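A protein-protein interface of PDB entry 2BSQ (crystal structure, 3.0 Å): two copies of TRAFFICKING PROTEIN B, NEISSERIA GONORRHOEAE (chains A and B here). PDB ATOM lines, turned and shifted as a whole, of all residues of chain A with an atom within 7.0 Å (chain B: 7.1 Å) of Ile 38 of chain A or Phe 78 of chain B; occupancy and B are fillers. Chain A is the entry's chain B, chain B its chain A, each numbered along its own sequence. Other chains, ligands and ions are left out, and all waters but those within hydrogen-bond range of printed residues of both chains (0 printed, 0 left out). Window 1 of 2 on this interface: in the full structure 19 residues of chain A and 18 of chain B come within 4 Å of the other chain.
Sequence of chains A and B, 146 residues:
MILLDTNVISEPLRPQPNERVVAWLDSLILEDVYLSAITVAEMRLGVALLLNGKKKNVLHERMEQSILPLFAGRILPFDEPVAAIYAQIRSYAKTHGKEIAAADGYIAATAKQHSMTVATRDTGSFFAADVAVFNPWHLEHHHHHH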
ATOM      1  N   THR A   6      14.720 -26.739  21.973  1.00  0.00           N
ATOM      2  CA  THR A   6      13.984 -25.779  21.166  1.00  0.00           C
ATOM      3  C   THR A   6      12.489 -25.739  21.470  1.00  0.00           C
ATOM      4  O   THR A   6      11.956 -24.704  21.850  1.00  0.00           O
ATOM      5  CB  THR A   6      14.190 -26.073  19.677  1.00  0.00           C
ATOM      6  OG1 THR A   6      15.579 -26.351  19.440  1.00  0.00           O
ATOM      7  CG2 THR A   6      13.741 -24.881  18.833  1.00  0.00           C
ATOM      8  N   LEU A  35      21.400 -23.133  26.851  1.00  0.00           N
ATOM      9  CA  LEU A  35      20.865 -23.233  25.503  1.00  0.00           C
ATOM     10  C   LEU A  35      21.979 -23.637  24.562  1.00  0.00           C
ATOM     11  O   LEU A  35      23.148 -23.260  24.733  1.00  0.00           O
ATOM     12  CB  LEU A  35      20.303 -21.904  25.026  1.00  0.00           C
ATOM     13  CG  LEU A  35      19.049 -21.441  25.732  1.00  0.00           C
ATOM     14  CD1 LEU A  35      18.789 -19.999  25.329  1.00  0.00           C
ATOM     15  CD2 LEU A  35      17.872 -22.372  25.394  1.00  0.00           C
ATOM     16  N   SER A  36      21.617 -24.414  23.559  1.00  0.00           N
ATOM     17  CA  SER A  36      22.600 -24.827  22.602  1.00  0.00           C
ATOM     18  C   SER A  36      22.633 -23.792  21.514  1.00  0.00           C
ATOM     19  O   SER A  36      21.597 -23.253  21.145  1.00  0.00           O
ATOM     20  CB  SER A  36      22.214 -26.149  21.989  1.00  0.00           C
ATOM     21  OG  SER A  36      22.838 -26.259  20.732  1.00  0.00           O
ATOM     22  N   ALA A  37      23.821 -23.499  21.008  1.00  0.00           N
ATOM     23  CA  ALA A  37      23.931 -22.565  19.916  1.00  0.00           C
ATOM     24  C   ALA A  37      22.971 -23.077  18.830  1.00  0.00           C
ATOM     25  O   ALA A  37      22.247 -22.290  18.220  1.00  0.00           O
ATOM     26  CB  ALA A  37      25.338 -22.548  19.403  1.00  0.00           C
ATOM     27  N   ILE A  38      22.958 -24.392  18.605  1.00  0.00           N
ATOM     28  CA  ILE A  38      22.070 -24.990  17.606  1.00  0.00           C
ATOM     29  C   ILE A  38      20.628 -24.581  17.900  1.00  0.00           C
ATOM     30  O   ILE A  38      19.842 -24.316  16.985  1.00  0.00           O
ATOM     31  CB  ILE A  38      22.134 -26.541  17.618  1.00  0.00           C
ATOM     32  CG1 ILE A  38      23.547 -27.011  17.314  1.00  0.00           C
ATOM     33  CG2 ILE A  38      21.198 -27.119  16.580  1.00  0.00           C
ATOM     34  CD1 ILE A  38      24.051 -26.589  15.963  1.00  0.00           C
ATOM     35  N   THR A  39      20.276 -24.528  19.182  1.00  0.00           N
ATOM     36  CA  THR A  39      18.921 -24.159  19.554  1.00  0.00           C
ATOM     37  C   THR A  39      18.677 -22.674  19.363  1.00  0.00           C
ATOM     38  O   THR A  39      17.592 -22.271  18.941  1.00  0.00           O
ATOM     39  CB  THR A  39      18.612 -24.521  21.005  1.00  0.00           C
ATOM     40  OG1 THR A  39      18.800 -25.927  21.193  1.00  0.00           O
ATOM     41  CG2 THR A  39      17.171 -24.160  21.339  1.00  0.00           C
ATOM     42  N   VAL A  40      19.674 -21.854  19.682  1.00  0.00           N
ATOM     43  CA  VAL A  40      19.526 -20.412  19.516  1.00  0.00           C
ATOM     44  C   VAL A  40      19.410 -20.128  18.028  1.00  0.00           C
ATOM     45  O   VAL A  40      18.632 -19.275  17.615  1.00  0.00           O
ATOM     46  CB  VAL A  40      20.726 -19.635  20.095  1.00  0.00           C
ATOM     47  CG1 VAL A  40      20.586 -18.171  19.781  1.00  0.00           C
ATOM     48  CG2 VAL A  40      20.782 -19.810  21.593  1.00  0.00           C
ATOM     49  N   ALA A  41      20.178 -20.861  17.225  1.00  0.00           N
ATOM     50  CA  ALA A  41      20.149 -20.710  15.776  1.00  0.00           C
ATOM     51  C   ALA A  41      18.770 -21.056  15.226  1.00  0.00           C
ATOM     52  O   ALA A  41      18.309 -20.455  14.271  1.00  0.00           O
ATOM     53  CB  ALA A  41      21.196 -21.602  15.139  1.00  0.00           C
ATOM     54  N   GLU A  42      18.112 -22.038  15.826  1.00  0.00           N
ATOM     55  CA  GLU A  42      16.784 -22.421  15.376  1.00  0.00           C
ATOM     56  C   GLU A  42      15.773 -21.312  15.745  1.00  0.00           C
ATOM     57  O   GLU A  42      14.886 -20.995  14.965  1.00  0.00           O
ATOM     58  CB  GLU A  42      16.388 -23.754  16.022  1.00  0.00           C
ATOM     59  CG  GLU A  42      15.872 -24.839  15.055  1.00  0.00           C
ATOM     60  CD  GLU A  42      15.373 -26.119  15.790  1.00  0.00           C
ATOM     61  OE1 GLU A  42      16.175 -26.771  16.517  1.00  0.00           O
ATOM     62  OE2 GLU A  42      14.172 -26.473  15.639  1.00  0.00           O
ATOM     63  N   MET A  43      15.910 -20.720  16.932  1.00  0.00           N
ATOM     64  CA  MET A  43      15.011 -19.643  17.360  1.00  0.00           C
ATOM     65  C   MET A  43      15.189 -18.445  16.441  1.00  0.00           C
ATOM     66  O   MET A  43      14.223 -17.921  15.900  1.00  0.00           O
ATOM     67  CB  MET A  43      15.320 -19.181  18.791  1.00  0.00           C
ATOM     68  CG  MET A  43      15.221 -20.247  19.879  1.00  0.00           C
ATOM     69  SD  MET A  43      16.064 -19.757  21.436  1.00  0.00           S
ATOM     70  CE  MET A  43      14.789 -18.800  22.197  1.00  0.00           C
ATOM     71  N   ILE A  75      25.256 -20.003  26.377  1.00  0.00           N
ATOM     72  CA  ILE A  75      24.787 -20.558  25.119  1.00  0.00           C
ATOM     73  C   ILE A  75      25.935 -21.433  24.641  1.00  0.00           C
ATOM     74  O   ILE A  75      26.880 -20.961  24.007  1.00  0.00           O
ATOM     75  CB  ILE A  75      24.476 -19.455  24.103  1.00  0.00           C
ATOM     76  CG1 ILE A  75      23.263 -18.660  24.585  1.00  0.00           C
ATOM     77  CG2 ILE A  75      24.200 -20.054  22.747  1.00  0.00           C
ATOM     78  CD1 ILE A  75      22.884 -17.501  23.700  1.00  0.00           C
ATOM     79  N   LEU A  76      25.848 -22.713  24.987  1.00  0.00           N
ATOM     80  CA  LEU A  76      26.862 -23.709  24.665  1.00  0.00           C
ATOM     81  C   LEU A  76      27.099 -23.902  23.174  1.00  0.00           C
ATOM     82  O   LEU A  76      26.155 -23.986  22.388  1.00  0.00           O
ATOM     83  CB  LEU A  76      26.461 -25.037  25.293  1.00  0.00           C
ATOM     84  CG  LEU A  76      25.969 -24.892  26.730  1.00  0.00           C
ATOM     85  CD1 LEU A  76      25.646 -26.261  27.282  1.00  0.00           C
ATOM     86  CD2 LEU A  76      27.022 -24.187  27.573  1.00  0.00           C
ATOM     87  N   PRO A  77      28.377 -23.993  22.767  1.00  0.00           N
ATOM     88  CA  PRO A  77      28.777 -24.175  21.373  1.00  0.00           C
ATOM     89  C   PRO A  77      28.915 -25.649  21.020  1.00  0.00           C
ATOM     90  O   PRO A  77      29.188 -26.486  21.888  1.00  0.00           O
ATOM     91  CB  PRO A  77      30.118 -23.483  21.336  1.00  0.00           C
ATOM     92  CG  PRO A  77      30.719 -23.978  22.618  1.00  0.00           C
ATOM     93  CD  PRO A  77      29.571 -23.816  23.614  1.00  0.00           C
ATOM     94  N   PHE A  78      28.737 -25.960  19.744  1.00  0.00           N
ATOM     95  CA  PHE A  78      28.875 -27.326  19.282  1.00  0.00           C
ATOM     96  C   PHE A  78      30.282 -27.411  18.714  1.00  0.00           C
ATOM     97  O   PHE A  78      30.526 -26.964  17.605  1.00  0.00           O
ATOM     98  CB  PHE A  78      27.854 -27.616  18.189  1.00  0.00           C
ATOM     99  CG  PHE A  78      27.885 -29.024  17.699  1.00  0.00           C
ATOM    100  CD1 PHE A  78      27.261 -30.036  18.412  1.00  0.00           C
ATOM    101  CD2 PHE A  78      28.559 -29.349  16.530  1.00  0.00           C
ATOM    102  CE1 PHE A  78      27.305 -31.356  17.968  1.00  0.00           C
ATOM    103  CE2 PHE A  78      28.612 -30.670  16.075  1.00  0.00           C
ATOM    104  CZ  PHE A  78      27.985 -31.672  16.795  1.00  0.00           C
ATOM    105  N   ASP A  79      31.215 -27.955  19.489  1.00  0.00           N
ATOM    106  CA  ASP A  79      32.597 -28.079  19.042  1.00  0.00           C
ATOM    107  C   ASP A  79      33.077 -29.507  18.782  1.00  0.00           C
ATOM    108  O   ASP A  79      32.296 -30.456  18.811  1.00  0.00           O
ATOM    109  CB  ASP A  79      33.537 -27.414  20.039  1.00  0.00           C
ATOM    110  CG  ASP A  79      33.188 -27.732  21.482  1.00  0.00           C
ATOM    111  OD1 ASP A  79      33.048 -28.927  21.846  1.00  0.00           O
ATOM    112  OD2 ASP A  79      33.068 -26.764  22.263  1.00  0.00           O
ATOM    113  N   ALA A 102      19.346 -35.763  13.683  1.00  0.00           N
ATOM    114  CA  ALA A 102      20.552 -34.954  13.845  1.00  0.00           C
ATOM    115  C   ALA A 102      20.236 -33.771  14.746  1.00  0.00           C
ATOM    116  O   ALA A 102      20.991 -33.447  15.663  1.00  0.00           O
ATOM    117  CB  ALA A 102      21.025 -34.456  12.510  1.00  0.00           C
ATOM    118  N   ALA A 103      19.110 -33.130  14.477  1.00  0.00           N
ATOM    119  CA  ALA A 103      18.688 -31.993  15.268  1.00  0.00           C
ATOM    120  C   ALA A 103      18.799 -32.333  16.754  1.00  0.00           C
ATOM    121  O   ALA A 103      19.467 -31.632  17.521  1.00  0.00           O
ATOM    122  CB  ALA A 103      17.257 -31.637  14.915  1.00  0.00           C
ATOM    123  N   TYR A 106      22.407 -33.271  18.334  1.00  0.00           N
ATOM    124  CA  TYR A 106      23.214 -32.096  18.654  1.00  0.00           C
ATOM    125  C   TYR A 106      22.978 -31.629  20.086  1.00  0.00           C
ATOM    126  O   TYR A 106      23.920 -31.402  20.843  1.00  0.00           O
ATOM    127  CB  TYR A 106      22.867 -30.956  17.704  1.00  0.00           C
ATOM    128  CG  TYR A 106      23.172 -31.225  16.258  1.00  0.00           C
ATOM    129  CD1 TYR A 106      22.256 -30.872  15.266  1.00  0.00           C
ATOM    130  CD2 TYR A 106      24.383 -31.799  15.871  1.00  0.00           C
ATOM    131  CE1 TYR A 106      22.538 -31.082  13.913  1.00  0.00           C
ATOM    132  CE2 TYR A 106      24.675 -32.015  14.521  1.00  0.00           C
ATOM    133  CZ  TYR A 106      23.747 -31.652  13.549  1.00  0.00           C
ATOM    134  OH  TYR A 106      24.011 -31.841  12.215  1.00  0.00           O
ATOM    135  N   ILE A 107      21.710 -31.454  20.440  1.00  0.00           N
ATOM    136  CA  ILE A 107      21.342 -31.042  21.782  1.00  0.00           C
ATOM    137  C   ILE A 107      21.800 -32.146  22.734  1.00  0.00           C
ATOM    138  O   ILE A 107      22.493 -31.896  23.715  1.00  0.00           O
ATOM    139  CB  ILE A 107      19.823 -30.902  21.900  1.00  0.00           C
ATOM    140  CG1 ILE A 107      19.290 -30.077  20.728  1.00  0.00           C
ATOM    141  CG2 ILE A 107      19.460 -30.275  23.228  1.00  0.00           C
ATOM    142  CD1 ILE A 107      19.992 -28.754  20.531  1.00  0.00           C
ATOM    143  N   THR A 110      25.398 -32.364  23.452  1.00  0.00           N
ATOM    144  CA  THR A 110      25.774 -31.199  24.230  1.00  0.00           C
ATOM    145  C   THR A 110      25.414 -31.473  25.675  1.00  0.00           C
ATOM    146  O   THR A 110      26.264 -31.434  26.549  1.00  0.00           O
ATOM    147  CB  THR A 110      25.029 -29.934  23.749  1.00  0.00           C
ATOM    148  OG1 THR A 110      25.329 -29.695  22.365  1.00  0.00           O
ATOM    149  CG2 THR A 110      25.440 -28.721  24.586  1.00  0.00           C
ATOM    150  N   SER B  36      34.502 -27.762   9.796  1.00  0.00           N
ATOM    151  CA  SER B  36      33.476 -27.321  10.728  1.00  0.00           C
ATOM    152  C   SER B  36      33.231 -28.455  11.723  1.00  0.00           C
ATOM    153  O   SER B  36      33.297 -29.636  11.366  1.00  0.00           O
ATOM    154  CB  SER B  36      32.162 -27.013  10.017  1.00  0.00           C
ATOM    155  OG  SER B  36      31.150 -26.692  10.968  1.00  0.00           O
ATOM    156  N   ALA B  37      32.957 -28.102  12.974  1.00  0.00           N
ATOM    157  CA  ALA B  37      32.674 -29.105  13.989  1.00  0.00           C
ATOM    158  C   ALA B  37      31.587 -30.006  13.413  1.00  0.00           C
ATOM    159  O   ALA B  37      31.654 -31.227  13.549  1.00  0.00           O
ATOM    160  CB  ALA B  37      32.189 -28.442  15.267  1.00  0.00           C
ATOM    161  N   ILE B  38      30.600 -29.390  12.758  1.00  0.00           N
ATOM    162  CA  ILE B  38      29.504 -30.124  12.136  1.00  0.00           C
ATOM    163  C   ILE B  38      30.086 -31.184  11.228  1.00  0.00           C
ATOM    164  O   ILE B  38      29.702 -32.349  11.294  1.00  0.00           O
ATOM    165  CB  ILE B  38      28.621 -29.232  11.258  1.00  0.00           C
ATOM    166  CG1 ILE B  38      27.967 -28.142  12.096  1.00  0.00           C
ATOM    167  CG2 ILE B  38      27.535 -30.066  10.609  1.00  0.00           C
ATOM    168  CD1 ILE B  38      27.031 -28.684  13.162  1.00  0.00           C
ATOM    169  N   ILE B  75      39.380 -26.307  13.607  1.00  0.00           N
ATOM    170  CA  ILE B  75      38.064 -26.954  13.579  1.00  0.00           C
ATOM    171  C   ILE B  75      37.101 -25.929  14.182  1.00  0.00           C
ATOM    172  O   ILE B  75      37.140 -25.622  15.370  1.00  0.00           O
ATOM    173  CB  ILE B  75      38.073 -28.285  14.368  1.00  0.00           C
ATOM    174  CG1 ILE B  75      38.998 -29.264  13.642  1.00  0.00           C
ATOM    175  CG2 ILE B  75      36.655 -28.865  14.471  1.00  0.00           C
ATOM    176  CD1 ILE B  75      39.034 -30.633  14.230  1.00  0.00           C
ATOM    177  N   LEU B  76      36.249 -25.399  13.319  1.00  0.00           N
ATOM    178  CA  LEU B  76      35.330 -24.343  13.680  1.00  0.00           C
ATOM    179  C   LEU B  76      34.010 -24.722  14.313  1.00  0.00           C
ATOM    180  O   LEU B  76      33.152 -25.356  13.691  1.00  0.00           O
ATOM    181  CB  LEU B  76      35.069 -23.473  12.448  1.00  0.00           C
ATOM    182  CG  LEU B  76      36.336 -23.013  11.714  1.00  0.00           C
ATOM    183  CD1 LEU B  76      35.942 -22.236  10.471  1.00  0.00           C
ATOM    184  CD2 LEU B  76      37.206 -22.174  12.646  1.00  0.00           C
ATOM    185  N   PRO B  77      33.815 -24.285  15.564  1.00  0.00           N
ATOM    186  CA  PRO B  77      32.619 -24.532  16.364  1.00  0.00           C
ATOM    187  C   PRO B  77      31.452 -23.717  15.879  1.00  0.00           C
ATOM    188  O   PRO B  77      31.628 -22.646  15.313  1.00  0.00           O
ATOM    189  CB  PRO B  77      33.044 -24.079  17.741  1.00  0.00           C
ATOM    190  CG  PRO B  77      33.908 -22.912  17.422  1.00  0.00           C
ATOM    191  CD  PRO B  77      34.770 -23.455  16.319  1.00  0.00           C
ATOM    192  N   PHE B  78      30.256 -24.228  16.112  1.00  0.00           N
ATOM    193  CA  PHE B  78      29.061 -23.504  15.740  1.00  0.00           C
ATOM    194  C   PHE B  78      28.617 -22.771  17.006  1.00  0.00           C
ATOM    195  O   PHE B  78      27.760 -23.251  17.743  1.00  0.00           O
ATOM    196  CB  PHE B  78      27.973 -24.458  15.307  1.00  0.00           C
ATOM    197  CG  PHE B  78      26.756 -23.771  14.802  1.00  0.00           C
ATOM    198  CD1 PHE B  78      26.646 -23.430  13.456  1.00  0.00           C
ATOM    199  CD2 PHE B  78      25.711 -23.453  15.667  1.00  0.00           C
ATOM    200  CE1 PHE B  78      25.508 -22.788  12.976  1.00  0.00           C
ATOM    201  CE2 PHE B  78      24.570 -22.809  15.201  1.00  0.00           C
ATOM    202  CZ  PHE B  78      24.467 -22.477  13.853  1.00  0.00           C
ATOM    203  N   ASP B  79      29.230 -21.616  17.252  1.00  0.00           N
ATOM    204  CA  ASP B  79      28.950 -20.784  18.415  1.00  0.00           C
ATOM    205  C   ASP B  79      27.771 -19.827  18.194  1.00  0.00           C
ATOM    206  O   ASP B  79      27.279 -19.697  17.072  1.00  0.00           O
ATOM    207  CB  ASP B  79      30.208 -19.987  18.760  1.00  0.00           C
ATOM    208  CG  ASP B  79      30.794 -19.254  17.548  1.00  0.00           C
ATOM    209  OD1 ASP B  79      30.025 -18.556  16.845  1.00  0.00           O
ATOM    210  OD2 ASP B  79      32.022 -19.363  17.296  1.00  0.00           O
ATOM    211  N   GLU B  80      27.334 -19.155  19.264  1.00  0.00           N
ATOM    212  CA  GLU B  80      26.208 -18.202  19.207  1.00  0.00           C
ATOM    213  C   GLU B  80      26.300 -17.170  18.062  1.00  0.00           C
ATOM    214  O   GLU B  80      25.311 -16.906  17.358  1.00  0.00           O
ATOM    215  CB  GLU B  80      26.064 -17.478  20.560  1.00  0.00           C
ATOM    216  CG  GLU B  80      24.990 -16.381  20.619  1.00  0.00           C
ATOM    217  CD  GLU B  80      25.450 -15.075  19.970  1.00  0.00           C
ATOM    218  OE1 GLU B  80      26.589 -14.649  20.261  1.00  0.00           O
ATOM    219  OE2 GLU B  80      24.686 -14.470  19.177  1.00  0.00           O
ATOM    220  N   PRO B  81      27.478 -16.549  17.881  1.00  0.00           N
ATOM    221  CA  PRO B  81      27.590 -15.576  16.797  1.00  0.00           C
ATOM    222  C   PRO B  81      27.181 -16.252  15.496  1.00  0.00           C
ATOM    223  O   PRO B  81      26.257 -15.810  14.808  1.00  0.00           O
ATOM    224  CB  PRO B  81      29.071 -15.231  16.798  1.00  0.00           C
ATOM    225  CG  PRO B  81      29.428 -15.351  18.227  1.00  0.00           C
ATOM    226  CD  PRO B  81      28.726 -16.612  18.660  1.00  0.00           C
ATOM    227  N   VAL B  82      27.859 -17.347  15.172  1.00  0.00           N
ATOM    228  CA  VAL B  82      27.561 -18.029  13.938  1.00  0.00           C
ATOM    229  C   VAL B  82      26.084 -18.266  13.770  1.00  0.00           C
ATOM    230  O   VAL B  82      25.574 -18.259  12.652  1.00  0.00           O
ATOM    231  CB  VAL B  82      28.262 -19.372  13.833  1.00  0.00           C
ATOM    232  CG1 VAL B  82      28.039 -19.942  12.447  1.00  0.00           C
ATOM    233  CG2 VAL B  82      29.735 -19.205  14.106  1.00  0.00           C
ATOM    234  N   ALA B  83      25.383 -18.468  14.869  1.00  0.00           N
ATOM    235  CA  ALA B  83      23.967 -18.732  14.751  1.00  0.00           C
ATOM    236  C   ALA B  83      23.246 -17.574  14.089  1.00  0.00           C
ATOM    237  O   ALA B  83      22.433 -17.769  13.192  1.00  0.00           O
ATOM    238  CB  ALA B  83      23.373 -19.018  16.118  1.00  0.00           C
ATOM    239  N   ALA B  84      23.550 -16.364  14.533  1.00  0.00           N
ATOM    240  CA  ALA B  84      22.910 -15.174  13.985  1.00  0.00           C
ATOM    241  C   ALA B  84      23.071 -15.152  12.477  1.00  0.00           C
ATOM    242  O   ALA B  84      22.117 -14.873  11.743  1.00  0.00           O
ATOM    243  CB  ALA B  84      23.526 -13.917  14.592  1.00  0.00           C
ATOM    244  N   TYR B  86      23.708 -17.714  10.503  1.00  0.00           N
ATOM    245  CA  TYR B  86      22.910 -18.824  10.004  1.00  0.00           C
ATOM    246  C   TYR B  86      21.471 -18.373   9.803  1.00  0.00           C
ATOM    247  O   TYR B  86      20.859 -18.645   8.773  1.00  0.00           O
ATOM    248  CB  TYR B  86      22.944 -19.965  11.014  1.00  0.00           C
ATOM    249  CG  TYR B  86      21.866 -21.002  10.834  1.00  0.00           C
ATOM    250  CD1 TYR B  86      22.017 -22.043   9.930  1.00  0.00           C
ATOM    251  CD2 TYR B  86      20.697 -20.950  11.597  1.00  0.00           C
ATOM    252  CE1 TYR B  86      21.034 -23.020   9.793  1.00  0.00           C
ATOM    253  CE2 TYR B  86      19.706 -21.914  11.470  1.00  0.00           C
ATOM    254  CZ  TYR B  86      19.881 -22.951  10.567  1.00  0.00           C
ATOM    255  OH  TYR B  86      18.912 -23.925  10.449  1.00  0.00           O
ATOM    256  N   ALA B  87      20.935 -17.678  10.798  1.00  0.00           N
ATOM    257  CA  ALA B  87      19.565 -17.203  10.721  1.00  0.00           C
ATOM    258  C   ALA B  87      19.318 -16.403   9.450  1.00  0.00           C
ATOM    259  O   ALA B  87      18.278 -16.561   8.807  1.00  0.00           O
ATOM    260  CB  ALA B  87      19.232 -16.360  11.946  1.00  0.00           C
ATOM    261  N   ALA B 102      19.365 -27.067   6.772  1.00  0.00           N
ATOM    262  CA  ALA B 102      20.050 -26.672   7.994  1.00  0.00           C
ATOM    263  C   ALA B 102      21.536 -27.046   8.021  1.00  0.00           C
ATOM    264  O   ALA B 102      22.391 -26.203   8.248  1.00  0.00           O
ATOM    265  CB  ALA B 102      19.341 -27.274   9.190  1.00  0.00           C
ATOM    266  N   GLY B 105      23.380 -24.955   6.015  1.00  0.00           N
ATOM    267  CA  GLY B 105      23.342 -23.602   6.527  1.00  0.00           C
ATOM    268  C   GLY B 105      24.384 -23.417   7.612  1.00  0.00           C
ATOM    269  O   GLY B 105      24.977 -22.348   7.744  1.00  0.00           O
ATOM    270  N   TYR B 106      24.607 -24.465   8.395  1.00  0.00           N
ATOM    271  CA  TYR B 106      25.573 -24.404   9.480  1.00  0.00           C
ATOM    272  C   TYR B 106      26.939 -24.165   8.862  1.00  0.00           C
ATOM    273  O   TYR B 106      27.662 -23.248   9.249  1.00  0.00           O
ATOM    274  CB  TYR B 106      25.553 -25.719  10.295  1.00  0.00           C
ATOM    275  CG  TYR B 106      24.249 -25.977  11.057  1.00  0.00           C
ATOM    276  CD1 TYR B 106      23.851 -27.277  11.396  1.00  0.00           C
ATOM    277  CD2 TYR B 106      23.406 -24.925  11.411  1.00  0.00           C
ATOM    278  CE1 TYR B 106      22.648 -27.520  12.062  1.00  0.00           C
ATOM    279  CE2 TYR B 106      22.200 -25.157  12.075  1.00  0.00           C
ATOM    280  CZ  TYR B 106      21.827 -26.452  12.398  1.00  0.00           C
ATOM    281  OH  TYR B 106      20.631 -26.653  13.053  1.00  0.00           O
ATOM    282  N   ILE B 107      27.272 -24.984   7.873  1.00  0.00           N
ATOM    283  CA  ILE B 107      28.551 -24.871   7.188  1.00  0.00           C
ATOM    284  C   ILE B 107      28.710 -23.499   6.535  1.00  0.00           C
ATOM    285  O   ILE B 107      29.713 -22.827   6.748  1.00  0.00           O
ATOM    286  CB  ILE B 107      28.718 -26.002   6.115  1.00  0.00           C
ATOM    287  CG1 ILE B 107      29.223 -27.299   6.772  1.00  0.00           C
ATOM    288  CG2 ILE B 107      29.706 -25.573   5.047  1.00  0.00           C
ATOM    289  CD1 ILE B 107      28.278 -27.906   7.790  1.00  0.00           C
ATOM    290  N   ALA B 109      27.020 -20.633   7.034  1.00  0.00           N
ATOM    291  CA  ALA B 109      27.073 -19.661   8.099  1.00  0.00           C
ATOM    292  C   ALA B 109      28.454 -19.645   8.724  1.00  0.00           C
ATOM    293  O   ALA B 109      29.038 -18.580   8.890  1.00  0.00           O
ATOM    294  CB  ALA B 109      26.021 -19.976   9.141  1.00  0.00           C
ATOM    295  N   THR B 110      28.984 -20.812   9.070  1.00  0.00           N
ATOM    296  CA  THR B 110      30.313 -20.852   9.668  1.00  0.00           C
ATOM    297  C   THR B 110      31.303 -20.162   8.726  1.00  0.00           C
ATOM    298  O   THR B 110      31.914 -19.157   9.082  1.00  0.00           O
ATOM    299  CB  THR B 110      30.779 -22.294   9.921  1.00  0.00           C
ATOM    300  OG1 THR B 110      29.924 -22.911  10.885  1.00  0.00           O
ATOM    301  CG2 THR B 110      32.195 -22.309  10.454  1.00  0.00           C
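The backbone carbonyl oxygen of Phe 78 of chain A sits at hydrogen-bond distance from the backbone NH of Phe 78 of chain B (3.1 Å).
N of Ala 37 of chain B sits at hydrogen-bond distance from O of Leu 76 of chain B (2.8 Å).
The backbone carbonyl oxygen (O) of Tyr 106 of chain B sits at hydrogen-bond distance from the side-chain hydroxyl (OG1) of Thr 110 of chain B (2.8 Å).
OG of Ser 36 of chain A is in hydrogen-bond range of N of Ile 38 of chain A (2.8 Å).
The side-chain hydroxyl of Ser 36 of chain B sits close to the backbone NH of Ile 38 of chain B (3.3 Å).
The backbone NH (N) of Ala 37 of chain A sits at hydrogen-bond distance from the backbone carbonyl oxygen (O) of Leu 76 of chain A (2.8 Å).
Of chain B, only Phe 78 (3.6 Å) and Tyr 106 (3.6 Å) come within 4 Å of Ile 38 of chain A.
Phe 78 of chain B touches five residues of chain A.
Ala 37 of chain A touches just these residues of chain B: Phe 78, Asp 79 and Glu 80.
Printed residues of chain A within 4 Å of Pro 77 of chain B: Phe 78.
Of the printed residues of chain A, Glu 80 of chain B touches Ala 37 (3.9 Å) and Ile 75 (3.9 Å).
Of the printed residues of chain B, Pro 77 of chain A touches Phe 78 (3.9 Å).
Printed residues of chain A within 4 Å of Ala 83 of chain B: Ala 41.
Printed residues of chain A within 4 Å of Asp 79 of chain B: Ala 37.
Ala 84 of chain B touches none of the printed residues of chain A.
The nearest residue of chain A that does not touch Phe 78 of chain B is Leu 76 of chain A (5.0 Å).
Printed residues of chain B that touch a printed residue of chain A: Ala 37, Ile 38, Pro 77, Phe 78, Asp 79, Glu 80, Ala 83, Tyr 86 and Tyr 106.
Hydrophobic or aromatic side chains of chain B that line the printed part of chain A: Ala 37, Ile 38, Pro 77, Phe 78, Ala 83, Tyr 86 and Tyr 106.
Hydrophobic or aromatic side chains of chain A that line the printed part of chain B: Ala 37, Ile 38, Ala 41, Ile 75 and Phe 78.
Along chain A the printed residues that touch a printed residue of chain B span positions 37 to 79.
Among the printed residues, 15 pairs touch across the chains.
Ala 37 of chain A touches Phe 78 of chain B, and with the chains exchanged Phe 78 of chain A touches Ala 37 of chain B.
Ala 37 of chain A touches Asp 79 of chain B, and with the chains exchanged Asp 79 of chain A touches Ala 37 of chain B.
Ile 38 of chain A touches Tyr 106 of chain B, but with the chains exchanged Tyr 106 of chain A does not touch Ile 38 of chain B (4.3 Å).
Pro 77 of chain A touches Phe 78 of chain B, and with the chains exchanged Phe 78 of chain A touches Pro 77 of chain B.
Positions printed for both chains: 36, 37, 38, 75, 76, 77, 78, 79, 102, 106, 107 and 110.
CB of Ala 37 of chain A touches O of Phe 78 of chain B (3.0 Å).
CB of Ala 37 of chain A touches C of Asp 79 of chain B, 3.8 Å away.
Ile 38 of chain A touches Phe 78 of chain B (CD1 to CD2, 3.6 Å).
Ile 38 of chain A touches Tyr 106 of chain B.
Ala 41 of chain A touches Ala 83 of chain B (CB to CB, 3.5 Å).
Ile 75 of chain A touches Glu 80 of chain B (CG2 to CB, 3.9 Å).
Pro 77 of chain A touches Phe 78 of chain B.
CD2 of Phe 78 of chain A touches CD1 of Ile 38 of chain B, at 3.8 Å.
Phe 78 of chain A touches Pro 77 of chain B (O to CA, 3.4 Å).
C of Asp 79 of chain A touches CB of Ala 37 of chain B, 3.8 Å away.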
